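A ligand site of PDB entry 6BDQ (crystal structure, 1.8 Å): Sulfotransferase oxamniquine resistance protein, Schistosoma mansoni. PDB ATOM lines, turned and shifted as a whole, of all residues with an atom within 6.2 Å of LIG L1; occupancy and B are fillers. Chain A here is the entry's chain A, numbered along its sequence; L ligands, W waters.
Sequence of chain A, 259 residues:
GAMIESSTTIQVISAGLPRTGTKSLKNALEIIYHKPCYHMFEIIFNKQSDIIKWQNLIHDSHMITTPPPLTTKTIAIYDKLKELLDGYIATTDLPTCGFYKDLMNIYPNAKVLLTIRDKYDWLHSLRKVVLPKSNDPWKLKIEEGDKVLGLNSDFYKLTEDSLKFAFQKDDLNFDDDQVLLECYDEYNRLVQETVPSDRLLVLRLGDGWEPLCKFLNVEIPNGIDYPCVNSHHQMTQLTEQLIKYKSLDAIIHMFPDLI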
ATOM      1  N   PRO A  18     -25.055   0.559  21.798  1.00  0.00           N
ATOM      2  CA  PRO A  18     -24.111   0.434  22.918  1.00  0.00           C
ATOM      3  C   PRO A  18     -23.058   1.530  22.848  1.00  0.00           C
ATOM      4  O   PRO A  18     -22.705   1.993  21.760  1.00  0.00           O
ATOM      5  CB  PRO A  18     -23.471  -0.958  22.682  1.00  0.00           C
ATOM      6  CG  PRO A  18     -23.730  -1.263  21.230  1.00  0.00           C
ATOM      7  CD  PRO A  18     -25.084  -0.660  20.964  1.00  0.00           C
ATOM      8  N   ARG A  19     -22.571   1.955  24.015  1.00  0.00           N
ATOM      9  CA  ARG A  19     -21.583   3.031  24.140  1.00  0.00           C
ATOM     10  C   ARG A  19     -22.165   4.420  23.893  1.00  0.00           C
ATOM     11  O   ARG A  19     -21.424   5.351  23.551  1.00  0.00           O
ATOM     12  CB  ARG A  19     -20.286   2.795  23.318  1.00  0.00           C
ATOM     13  CG  ARG A  19     -19.728   1.354  23.448  1.00  0.00           C
ATOM     14  CD  ARG A  19     -19.576   0.936  24.925  1.00  0.00           C
ATOM     15  NE  ARG A  19     -18.638   1.793  25.641  1.00  0.00           N
ATOM     16  CZ  ARG A  19     -18.408   1.741  26.953  1.00  0.00           C
ATOM     17  NH1 ARG A  19     -19.077   0.874  27.714  1.00  0.00           N
ATOM     18  NH2 ARG A  19     -17.507   2.553  27.513  1.00  0.00           N
ATOM     19  N   THR A  22     -25.928   3.837  27.751  1.00  0.00           N
ATOM     20  CA  THR A  22     -27.032   2.948  28.069  1.00  0.00           C
ATOM     21  C   THR A  22     -27.006   2.480  29.520  1.00  0.00           C
ATOM     22  O   THR A  22     -28.058   2.326  30.132  1.00  0.00           O
ATOM     23  CB  THR A  22     -27.084   1.739  27.117  1.00  0.00           C
ATOM     24  OG1 THR A  22     -25.889   0.980  27.262  1.00  0.00           O
ATOM     25  CG2 THR A  22     -27.260   2.179  25.664  1.00  0.00           C
ATOM     26  N   HIS A  39     -30.649  -4.610  29.785  1.00  0.00           N
ATOM     27  CA  HIS A  39     -29.340  -4.141  29.329  1.00  0.00           C
ATOM     28  C   HIS A  39     -28.517  -5.401  29.107  1.00  0.00           C
ATOM     29  O   HIS A  39     -28.843  -6.469  29.638  1.00  0.00           O
ATOM     30  CB  HIS A  39     -28.686  -3.267  30.405  1.00  0.00           C
ATOM     31  CG  HIS A  39     -27.414  -2.598  29.981  1.00  0.00           C
ATOM     32  ND1 HIS A  39     -26.168  -3.175  30.148  1.00  0.00           N
ATOM     33  CD2 HIS A  39     -27.179  -1.375  29.450  1.00  0.00           C
ATOM     34  CE1 HIS A  39     -25.237  -2.355  29.703  1.00  0.00           C
ATOM     35  NE2 HIS A  39     -25.817  -1.253  29.273  1.00  0.00           N
ATOM     36  N   MET A  40     -27.432  -5.296  28.333  1.00  0.00           N
ATOM     37  CA  MET A  40     -26.573  -6.467  28.172  1.00  0.00           C
ATOM     38  C   MET A  40     -26.054  -6.982  29.524  1.00  0.00           C
ATOM     39  O   MET A  40     -25.883  -8.189  29.710  1.00  0.00           O
ATOM     40  CB  MET A  40     -25.417  -6.170  27.217  1.00  0.00           C
ATOM     41  CG  MET A  40     -24.548  -7.394  26.885  1.00  0.00           C
ATOM     42  SD  MET A  40     -25.508  -8.697  26.066  1.00  0.00           S
ATOM     43  CE  MET A  40     -25.328  -8.231  24.355  1.00  0.00           C
ATOM     44  N   PHE A  41     -25.839  -6.078  30.490  1.00  0.00           N
ATOM     45  CA  PHE A  41     -25.353  -6.488  31.809  1.00  0.00           C
ATOM     46  C   PHE A  41     -26.370  -7.338  32.561  1.00  0.00           C
ATOM     47  O   PHE A  41     -25.975  -8.133  33.416  1.00  0.00           O
ATOM     48  CB  PHE A  41     -25.011  -5.258  32.659  1.00  0.00           C
ATOM     49  CG  PHE A  41     -23.721  -4.577  32.276  1.00  0.00           C
ATOM     50  CD1 PHE A  41     -23.174  -4.766  31.016  1.00  0.00           C
ATOM     51  CD2 PHE A  41     -23.068  -3.752  33.173  1.00  0.00           C
ATOM     52  CE1 PHE A  41     -21.980  -4.119  30.656  1.00  0.00           C
ATOM     53  CE2 PHE A  41     -21.885  -3.101  32.804  1.00  0.00           C
ATOM     54  CZ  PHE A  41     -21.349  -3.298  31.545  1.00  0.00           C
ATOM     55  N   ILE A  44     -25.404 -10.641  31.270  1.00  0.00           N
ATOM     56  CA  ILE A  44     -24.104 -11.085  31.767  1.00  0.00           C
ATOM     57  C   ILE A  44     -24.196 -11.528  33.221  1.00  0.00           C
ATOM     58  O   ILE A  44     -23.706 -12.594  33.603  1.00  0.00           O
ATOM     59  CB  ILE A  44     -23.053  -9.985  31.586  1.00  0.00           C
ATOM     60  CG1 ILE A  44     -22.736  -9.774  30.100  1.00  0.00           C
ATOM     61  CG2 ILE A  44     -21.804 -10.331  32.364  1.00  0.00           C
ATOM     62  CD1 ILE A  44     -21.935  -8.519  29.790  1.00  0.00           C
ATOM     63  N   PHE A  45     -24.800 -10.697  34.071  1.00  0.00           N
ATOM     64  CA  PHE A  45     -24.710 -10.899  35.504  1.00  0.00           C
ATOM     65  C   PHE A  45     -25.908 -11.609  36.119  1.00  0.00           C
ATOM     66  O   PHE A  45     -25.771 -12.179  37.201  1.00  0.00           O
ATOM     67  CB  PHE A  45     -24.467  -9.566  36.205  1.00  0.00           C
ATOM     68  CG  PHE A  45     -23.187  -8.921  35.797  1.00  0.00           C
ATOM     69  CD1 PHE A  45     -21.969  -9.434  36.240  1.00  0.00           C
ATOM     70  CD2 PHE A  45     -23.173  -7.807  34.964  1.00  0.00           C
ATOM     71  CE1 PHE A  45     -20.771  -8.845  35.851  1.00  0.00           C
ATOM     72  CE2 PHE A  45     -21.985  -7.217  34.576  1.00  0.00           C
ATOM     73  CZ  PHE A  45     -20.776  -7.727  35.020  1.00  0.00           C
ATOM     74  N   ASP A  93     -29.825  -1.023  25.128  1.00  0.00           N
ATOM     75  CA  ASP A  93     -28.582  -1.718  24.771  1.00  0.00           C
ATOM     76  C   ASP A  93     -28.829  -2.899  23.850  1.00  0.00           C
ATOM     77  O   ASP A  93     -29.984  -3.283  23.616  1.00  0.00           O
ATOM     78  CB  ASP A  93     -27.854  -2.177  26.053  1.00  0.00           C
ATOM     79  CG  ASP A  93     -26.388  -2.568  25.834  1.00  0.00           C
ATOM     80  OD1 ASP A  93     -25.822  -2.319  24.749  1.00  0.00           O
ATOM     81  OD2 ASP A  93     -25.799  -3.118  26.780  1.00  0.00           O
ATOM     82  N   LEU A  94     -27.760  -3.491  23.310  1.00  0.00           N
ATOM     83  CA  LEU A  94     -27.877  -4.812  22.701  1.00  0.00           C
ATOM     84  C   LEU A  94     -28.295  -5.826  23.775  1.00  0.00           C
ATOM     85  O   LEU A  94     -27.927  -5.685  24.951  1.00  0.00           O
ATOM     86  CB  LEU A  94     -26.521  -5.249  22.140  1.00  0.00           C
ATOM     87  CG  LEU A  94     -25.802  -4.389  21.100  1.00  0.00           C
ATOM     88  CD1 LEU A  94     -24.399  -4.941  20.801  1.00  0.00           C
ATOM     89  CD2 LEU A  94     -26.629  -4.300  19.813  1.00  0.00           C
ATOM     90  N   VAL A 129     -14.099  -1.515  24.154  1.00  0.00           N
ATOM     91  CA  VAL A 129     -15.001  -2.206  25.082  1.00  0.00           C
ATOM     92  C   VAL A 129     -15.684  -3.406  24.427  1.00  0.00           C
ATOM     93  O   VAL A 129     -15.715  -4.503  24.990  1.00  0.00           O
ATOM     94  CB  VAL A 129     -16.025  -1.242  25.702  1.00  0.00           C
ATOM     95  CG1 VAL A 129     -16.986  -2.011  26.614  1.00  0.00           C
ATOM     96  CG2 VAL A 129     -15.315  -0.125  26.475  1.00  0.00           C
ATOM     97  N   VAL A 130     -16.270  -3.208  23.247  1.00  0.00           N
ATOM     98  CA  VAL A 130     -17.194  -4.167  22.657  1.00  0.00           C
ATOM     99  C   VAL A 130     -16.564  -4.890  21.475  1.00  0.00           C
ATOM    100  O   VAL A 130     -16.720  -6.107  21.332  1.00  0.00           O
ATOM    101  CB  VAL A 130     -18.508  -3.480  22.227  1.00  0.00           C
ATOM    102  CG1 VAL A 130     -19.470  -4.482  21.563  1.00  0.00           C
ATOM    103  CG2 VAL A 130     -19.176  -2.789  23.407  1.00  0.00           C
ATOM    104  N   ILE A 142      -9.740  -8.853  26.841  1.00  0.00           N
ATOM    105  CA  ILE A 142     -11.197  -8.879  26.999  1.00  0.00           C
ATOM    106  C   ILE A 142     -11.685 -10.316  27.053  1.00  0.00           C
ATOM    107  O   ILE A 142     -12.529 -10.677  27.882  1.00  0.00           O
ATOM    108  CB  ILE A 142     -11.893  -8.069  25.897  1.00  0.00           C
ATOM    109  CG1 ILE A 142     -11.477  -6.588  25.946  1.00  0.00           C
ATOM    110  CG2 ILE A 142     -13.402  -8.185  26.036  1.00  0.00           C
ATOM    111  CD1 ILE A 142     -12.110  -5.757  24.822  1.00  0.00           C
ATOM    112  N   GLY A 145     -10.905 -11.896  30.571  1.00  0.00           N
ATOM    113  CA  GLY A 145     -11.851 -11.463  31.585  1.00  0.00           C
ATOM    114  C   GLY A 145     -13.225 -12.082  31.386  1.00  0.00           C
ATOM    115  O   GLY A 145     -13.916 -12.424  32.357  1.00  0.00           O
ATOM    116  N   ASP A 146     -13.653 -12.221  30.134  1.00  0.00           N
ATOM    117  CA  ASP A 146     -14.976 -12.813  29.884  1.00  0.00           C
ATOM    118  C   ASP A 146     -15.054 -14.254  30.391  1.00  0.00           C
ATOM    119  O   ASP A 146     -16.087 -14.670  30.923  1.00  0.00           O
ATOM    120  CB  ASP A 146     -15.280 -12.773  28.394  1.00  0.00           C
ATOM    121  CG  ASP A 146     -15.759 -11.411  27.933  1.00  0.00           C
ATOM    122  OD1 ASP A 146     -16.041 -10.583  28.817  1.00  0.00           O
ATOM    123  OD2 ASP A 146     -15.831 -11.187  26.704  1.00  0.00           O
ATOM    124  N   LEU A 149     -16.163 -14.548  33.837  1.00  0.00           N
ATOM    125  CA  LEU A 149     -17.597 -14.375  34.012  1.00  0.00           C
ATOM    126  C   LEU A 149     -18.413 -15.554  33.503  1.00  0.00           C
ATOM    127  O   LEU A 149     -19.648 -15.547  33.657  1.00  0.00           O
ATOM    128  CB  LEU A 149     -18.038 -13.093  33.302  1.00  0.00           C
ATOM    129  CG  LEU A 149     -17.428 -11.803  33.865  1.00  0.00           C
ATOM    130  CD1 LEU A 149     -17.913 -10.582  33.059  1.00  0.00           C
ATOM    131  CD2 LEU A 149     -17.795 -11.651  35.337  1.00  0.00           C
ATOM    132  N   LEU A 151     -18.459 -16.355  30.216  1.00  0.00           N
ATOM    133  CA  LEU A 151     -18.834 -15.986  28.861  1.00  0.00           C
ATOM    134  C   LEU A 151     -17.832 -16.546  27.855  1.00  0.00           C
ATOM    135  O   LEU A 151     -16.618 -16.461  28.071  1.00  0.00           O
ATOM    136  CB  LEU A 151     -18.883 -14.461  28.722  1.00  0.00           C
ATOM    137  CG  LEU A 151     -19.766 -13.721  29.725  1.00  0.00           C
ATOM    138  CD1 LEU A 151     -19.414 -12.232  29.740  1.00  0.00           C
ATOM    139  CD2 LEU A 151     -21.244 -13.929  29.402  1.00  0.00           C
ATOM    140  N   PHE A 155     -21.580 -15.975  23.748  1.00  0.00           N
ATOM    141  CA  PHE A 155     -21.829 -14.578  24.073  1.00  0.00           C
ATOM    142  C   PHE A 155     -21.266 -13.658  22.994  1.00  0.00           C
ATOM    143  O   PHE A 155     -21.866 -12.619  22.688  1.00  0.00           O
ATOM    144  CB  PHE A 155     -21.205 -14.250  25.438  1.00  0.00           C
ATOM    145  CG  PHE A 155     -21.324 -12.806  25.820  1.00  0.00           C
ATOM    146  CD1 PHE A 155     -22.518 -12.293  26.308  1.00  0.00           C
ATOM    147  CD2 PHE A 155     -20.235 -11.948  25.692  1.00  0.00           C
ATOM    148  CE1 PHE A 155     -22.629 -10.940  26.656  1.00  0.00           C
ATOM    149  CE2 PHE A 155     -20.338 -10.607  26.038  1.00  0.00           C
ATOM    150  CZ  PHE A 155     -21.536 -10.102  26.515  1.00  0.00           C
ATOM    151  N   THR A 159     -23.395 -10.842  20.721  1.00  0.00           N
ATOM    152  CA  THR A 159     -22.998  -9.446  20.577  1.00  0.00           C
ATOM    153  C   THR A 159     -22.878  -9.060  19.113  1.00  0.00           C
ATOM    154  O   THR A 159     -23.516  -8.115  18.644  1.00  0.00           O
ATOM    155  CB  THR A 159     -21.681  -9.204  21.324  1.00  0.00           C
ATOM    156  OG1 THR A 159     -21.850  -9.538  22.709  1.00  0.00           O
ATOM    157  CG2 THR A 159     -21.265  -7.746  21.228  1.00  0.00           C
ATOM    158  N   ASN A 230     -19.657   3.335  33.494  1.00  0.00           N
ATOM    159  CA  ASN A 230     -19.387   2.504  32.327  1.00  0.00           C
ATOM    160  C   ASN A 230     -18.501   3.184  31.277  1.00  0.00           C
ATOM    161  O   ASN A 230     -18.591   2.860  30.082  1.00  0.00           O
ATOM    162  CB  ASN A 230     -20.673   1.939  31.713  1.00  0.00           C
ATOM    163  CG  ASN A 230     -20.422   0.635  30.975  1.00  0.00           C
ATOM    164  OD1 ASN A 230     -19.453  -0.050  31.261  1.00  0.00           O
ATOM    165  ND2 ASN A 230     -21.277   0.307  30.015  1.00  0.00           N
ATOM    166  N   SME A 235     -14.270   0.079  32.228  1.00  0.00           N
ATOM    167  CA  SME A 235     -14.407  -1.225  31.603  1.00  0.00           C
ATOM    168  CB  SME A 235     -15.051  -1.234  30.196  1.00  0.00           C
ATOM    169  CG  SME A 235     -16.519  -0.864  30.260  1.00  0.00           C
ATOM    170  S   SME A 235     -17.551  -2.318  30.347  1.00  0.00           S
ATOM    171  OE  SME A 235     -16.723  -3.437  29.822  1.00  0.00           O
ATOM    172  CE  SME A 235     -17.694  -2.555  32.058  1.00  0.00           C
ATOM    173  C   SME A 235     -13.040  -1.921  31.520  1.00  0.00           C
ATOM    174  O   SME A 235     -12.845  -3.113  31.706  1.00  0.00           O
ATOM    175  N   LEU A 238     -12.242  -3.152  35.016  1.00  0.00           N
ATOM    176  CA  LEU A 238     -12.970  -4.389  35.302  1.00  0.00           C
ATOM    177  C   LEU A 238     -12.263  -5.591  34.673  1.00  0.00           C
ATOM    178  O   LEU A 238     -12.042  -6.611  35.328  1.00  0.00           O
ATOM    179  CB  LEU A 238     -14.415  -4.292  34.798  1.00  0.00           C
ATOM    180  CG  LEU A 238     -15.318  -5.517  34.969  1.00  0.00           C
ATOM    181  CD1 LEU A 238     -15.300  -5.974  36.422  1.00  0.00           C
ATOM    182  CD2 LEU A 238     -16.743  -5.205  34.514  1.00  0.00           C
ATOM    183  N   THR A 239     -11.900  -5.468  33.394  1.00  0.00           N
ATOM    184  CA  THR A 239     -11.230  -6.560  32.692  1.00  0.00           C
ATOM    185  C   THR A 239      -9.903  -6.919  33.361  1.00  0.00           C
ATOM    186  O   THR A 239      -9.606  -8.088  33.592  1.00  0.00           O
ATOM    187  CB  THR A 239     -11.016  -6.164  31.232  1.00  0.00           C
ATOM    188  OG1 THR A 239     -12.282  -6.147  30.548  1.00  0.00           O
ATOM    189  CG2 THR A 239     -10.042  -7.127  30.524  1.00  0.00           C
ATOM    190  N   LEU A 242     -10.699  -8.638  36.747  1.00  0.00           N
ATOM    191  CA  LEU A 242     -11.178 -10.005  36.567  1.00  0.00           C
ATOM    192  C   LEU A 242     -10.024 -10.955  36.252  1.00  0.00           C
ATOM    193  O   LEU A 242      -9.972 -12.075  36.774  1.00  0.00           O
ATOM    194  CB  LEU A 242     -12.220 -10.054  35.440  1.00  0.00           C
ATOM    195  CG  LEU A 242     -13.595  -9.467  35.741  1.00  0.00           C
ATOM    196  CD1 LEU A 242     -14.418  -9.265  34.460  1.00  0.00           C
ATOM    197  CD2 LEU A 242     -14.345 -10.357  36.749  1.00  0.00           C
HETATM  198  C1  LIG L   1     -21.240  -5.871  25.443  1.00  0.00           C
HETATM  199  C2  LIG L   1     -17.538  -6.665  28.467  1.00  0.00           C
HETATM  200  C3  LIG L   1     -18.502  -7.222  29.500  1.00  0.00           C
HETATM  201  C4  LIG L   1     -17.864  -7.373  30.875  1.00  0.00           C
HETATM  202  C5  LIG L   1     -16.581  -8.173  30.784  1.00  0.00           C
HETATM  203  C6  LIG L   1     -21.434  -4.574  25.891  1.00  0.00           C
HETATM  204  C7  LIG L   1     -16.233  -7.475  28.494  1.00  0.00           C
HETATM  205  C8  LIG L   1     -20.524  -4.003  26.790  1.00  0.00           C
HETATM  206  C9  LIG L   1     -19.419  -4.746  27.209  1.00  0.00           C
HETATM  207  C10 LIG L   1     -19.227  -6.054  26.770  1.00  0.00           C
HETATM  208  C11 LIG L   1     -20.144  -6.614  25.872  1.00  0.00           C
HETATM  209  C12 LIG L   1     -22.659  -3.854  25.367  1.00  0.00           C
HETATM  210  N1  LIG L   1     -18.153  -6.786  27.162  1.00  0.00           N
HETATM  211  N2  LIG L   1     -15.670  -7.484  29.855  1.00  0.00           N
HETATM  212  N3  LIG L   1     -20.626  -2.679  27.275  1.00  0.00           N
HETATM  213  O1  LIG L   1     -20.866  -1.734  26.510  1.00  0.00           O
HETATM  214  O2  LIG L   1     -20.417  -2.424  28.471  1.00  0.00           O
HETATM  215  O3  LIG L   1     -23.345  -3.265  26.483  1.00  0.00           O
HETATM  216  P1  LG2 L   2     -16.536   6.457  27.017  1.00  0.00           P
HETATM  217  O1  LG2 L   2     -16.207   7.374  25.886  1.00  0.00           O
HETATM  218  O2  LG2 L   2     -16.201   5.015  26.729  1.00  0.00           O
HETATM  219  O3  LG2 L   2     -16.073   6.903  28.382  1.00  0.00           O
HETATM  220  P2  LG2 L   2     -22.766   2.422  27.506  1.00  0.00           P
HETATM  221  O4  LG2 L   2     -23.917   2.592  26.562  1.00  0.00           O
HETATM  222  O5  LG2 L   2     -23.120   2.386  28.980  1.00  0.00           O
HETATM  223  O6  LG2 L   2     -21.748   1.397  27.130  1.00  0.00           O
HETATM  224  O7  LG2 L   2     -22.059   3.860  27.301  1.00  0.00           O
HETATM  225  C1  LG2 L   2     -20.893   4.219  28.047  1.00  0.00           C
HETATM  226  C2  LG2 L   2     -20.286   5.517  27.486  1.00  0.00           C
HETATM  227  O8  LG2 L   2     -21.115   6.615  27.857  1.00  0.00           O
HETATM  228  C3  LG2 L   2     -18.910   5.828  28.076  1.00  0.00           C
HETATM  229  O9  LG2 L   2     -18.157   6.569  27.107  1.00  0.00           O
HETATM  230  C4  LG2 L   2     -19.242   6.701  29.265  1.00  0.00           C
HETATM  231  O10 LG2 L   2     -18.131   7.515  29.686  1.00  0.00           O
HETATM  232  C5  LG2 L   2     -20.371   7.522  28.677  1.00  0.00           C
HETATM  233  N1  LG2 L   2     -21.295   8.051  29.703  1.00  0.00           N
HETATM  234  C6  LG2 L   2     -22.079   7.335  30.536  1.00  0.00           C
HETATM  235  N2  LG2 L   2     -22.801   8.167  31.346  1.00  0.00           N
HETATM  236  C7  LG2 L   2     -22.476   9.430  30.995  1.00  0.00           C
HETATM  237  C8  LG2 L   2     -22.854  10.779  31.436  1.00  0.00           C
HETATM  238  N3  LG2 L   2     -23.760  10.927  32.425  1.00  0.00           N
HETATM  239  N4  LG2 L   2     -22.271  11.841  30.832  1.00  0.00           N
HETATM  240  C9  LG2 L   2     -21.360  11.672  29.839  1.00  0.00           C
HETATM  241  N5  LG2 L   2     -20.952  10.473  29.378  1.00  0.00           N
HETATM  242  C10 LG2 L   2     -21.466   9.342  29.915  1.00  0.00           C
HETATM  243  O   HOH W   1     -23.091  -0.929  27.887  1.00  0.00           O
HETATM  244  O   HOH W   2     -15.172  -5.237  31.124  1.00  0.00           O
HETATM  245  O   HOH W   3     -13.242  -8.720  29.970  1.00  0.00           O
HETATM  246  O   HOH W   4     -15.013  -4.654  27.556  1.00  0.00           O
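The guanidinium group (NH1) of Arg 19 lies within salt-bridge range of an oxygen (O6) of LG2 L2. An oxygen (O4) of LG2 L2 is in hydrogen-bond range of the backbone NH of Arg 19. The backbone NH (N) of Thr 22 is in hydrogen-bond range of an oxygen (O4) of LG2 L2 (2.6 Å). The side-chain amide nitrogen (ND2) of Asn 230 lies within hydrogen-bond range of an oxygen (O5) of LG2 L2 (3.0 Å). O4 of LG2 L2 sits at hydrogen-bond distance from OG1 of Thr 22 (2.6 Å). The guanidinium group of Arg 19 lies close to an oxygen (O1) of LIG L1, at 3.4 Å. The side-chain carboxylate (OD2) of Asp 93 sits at hydrogen-bond distance from an oxygen (O3) of LIG L1 (2.5 Å). O2 of LIG L1 sits at hydrogen-bond distance from ND2 of Asn 230. N2 of LIG L1 lies within salt-bridge range of OD1 of Asp 146 (3.3 Å).
A ring nitrogen (NE2) of His 39 sits close to the side-chain carboxylate (OD2) of Asp 93. O of Phe 155 lies within hydrogen-bond range of OG1 of Thr 159 (3.1 Å). The backbone carbonyl oxygen (O) of Asn 230 is in hydrogen-bond range of the guanidinium group (NH2) of Arg 19, 2.8 Å away. NE2 of His 39 lies within hydrogen-bond range of OG1 of Thr 22 (3.0 Å). The backbone NH (N) of Phe 41 sits at hydrogen-bond distance from a ring nitrogen (ND1) of His 39. The backbone NH of Met 40 lies close to the side-chain carboxylate of Asp 93, 3.1 Å away. O of SME 235 lies within hydrogen-bond range of OG1 of Thr 239 (3.3 Å). The backbone NH (N) of Leu 151 sits at hydrogen-bond distance from the backbone carbonyl oxygen (O) of Asp 146 (3.0 Å).
Water W2 lies within hydrogen-bond range of a nitrogen (N2) of LIG L1 (2.6 Å), OE of SME 235 (2.7 Å) and the side-chain hydroxyl (OG1) of Thr 239 (3.1 Å). Water W3 lies within hydrogen-bond range of N2 of LIG L1 (2.7 Å), OG1 of Thr 239 (2.8 Å) and O of Ile 142 (2.9 Å). Water W1 lies within hydrogen-bond range of O3 of LIG L1, O6 of LG2 L2, ND2 of Asn 230, NE2 of His 39 and OG1 of Thr 22. Water W4 bridges O of Val 129 and OE of SME 235.
S of SME 235 lies close to O2 of LIG L1 (3.4 Å). CE1 of His 39 touches O3 of LIG L1 (3.8 Å). Met 40 touches LIG L1 (CB to O3, 3.6 Å). Phe 41 touches LIG L1 (CE1 to O2, 3.2 Å). Ile 44 touches LIG L1 (CD1 to C3, 3.7 Å). Val 129 touches LIG L1 (CG1 to C9, 3.7 Å). CG2 of Val 130 touches O1 of LIG L1, 3.7 Å away. Ile 142 touches LIG L1 (CG2 to C7, 3.8 Å). Leu 149 touches LIG L1. Phe 155 touches LIG L1 (CZ to C11, 3.8 Å). Thr 239 touches LIG L1. Hydrophobic or aromatic side chains within 4 Å of LIG L1: His 39, Met 40, Phe 41, Ile 44, Val 129, Val 130, Ile 142, Leu 149 and Phe 155. 15 residues have an atom within 4 Å of LIG L1: Arg 19, His 39, Met 40, Phe 41, Ile 44, Asp 93, Val 129, Val 130, Ile 142, Asp 146, Leu 149, Phe 155, Asn 230, SME 235 and Thr 239.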
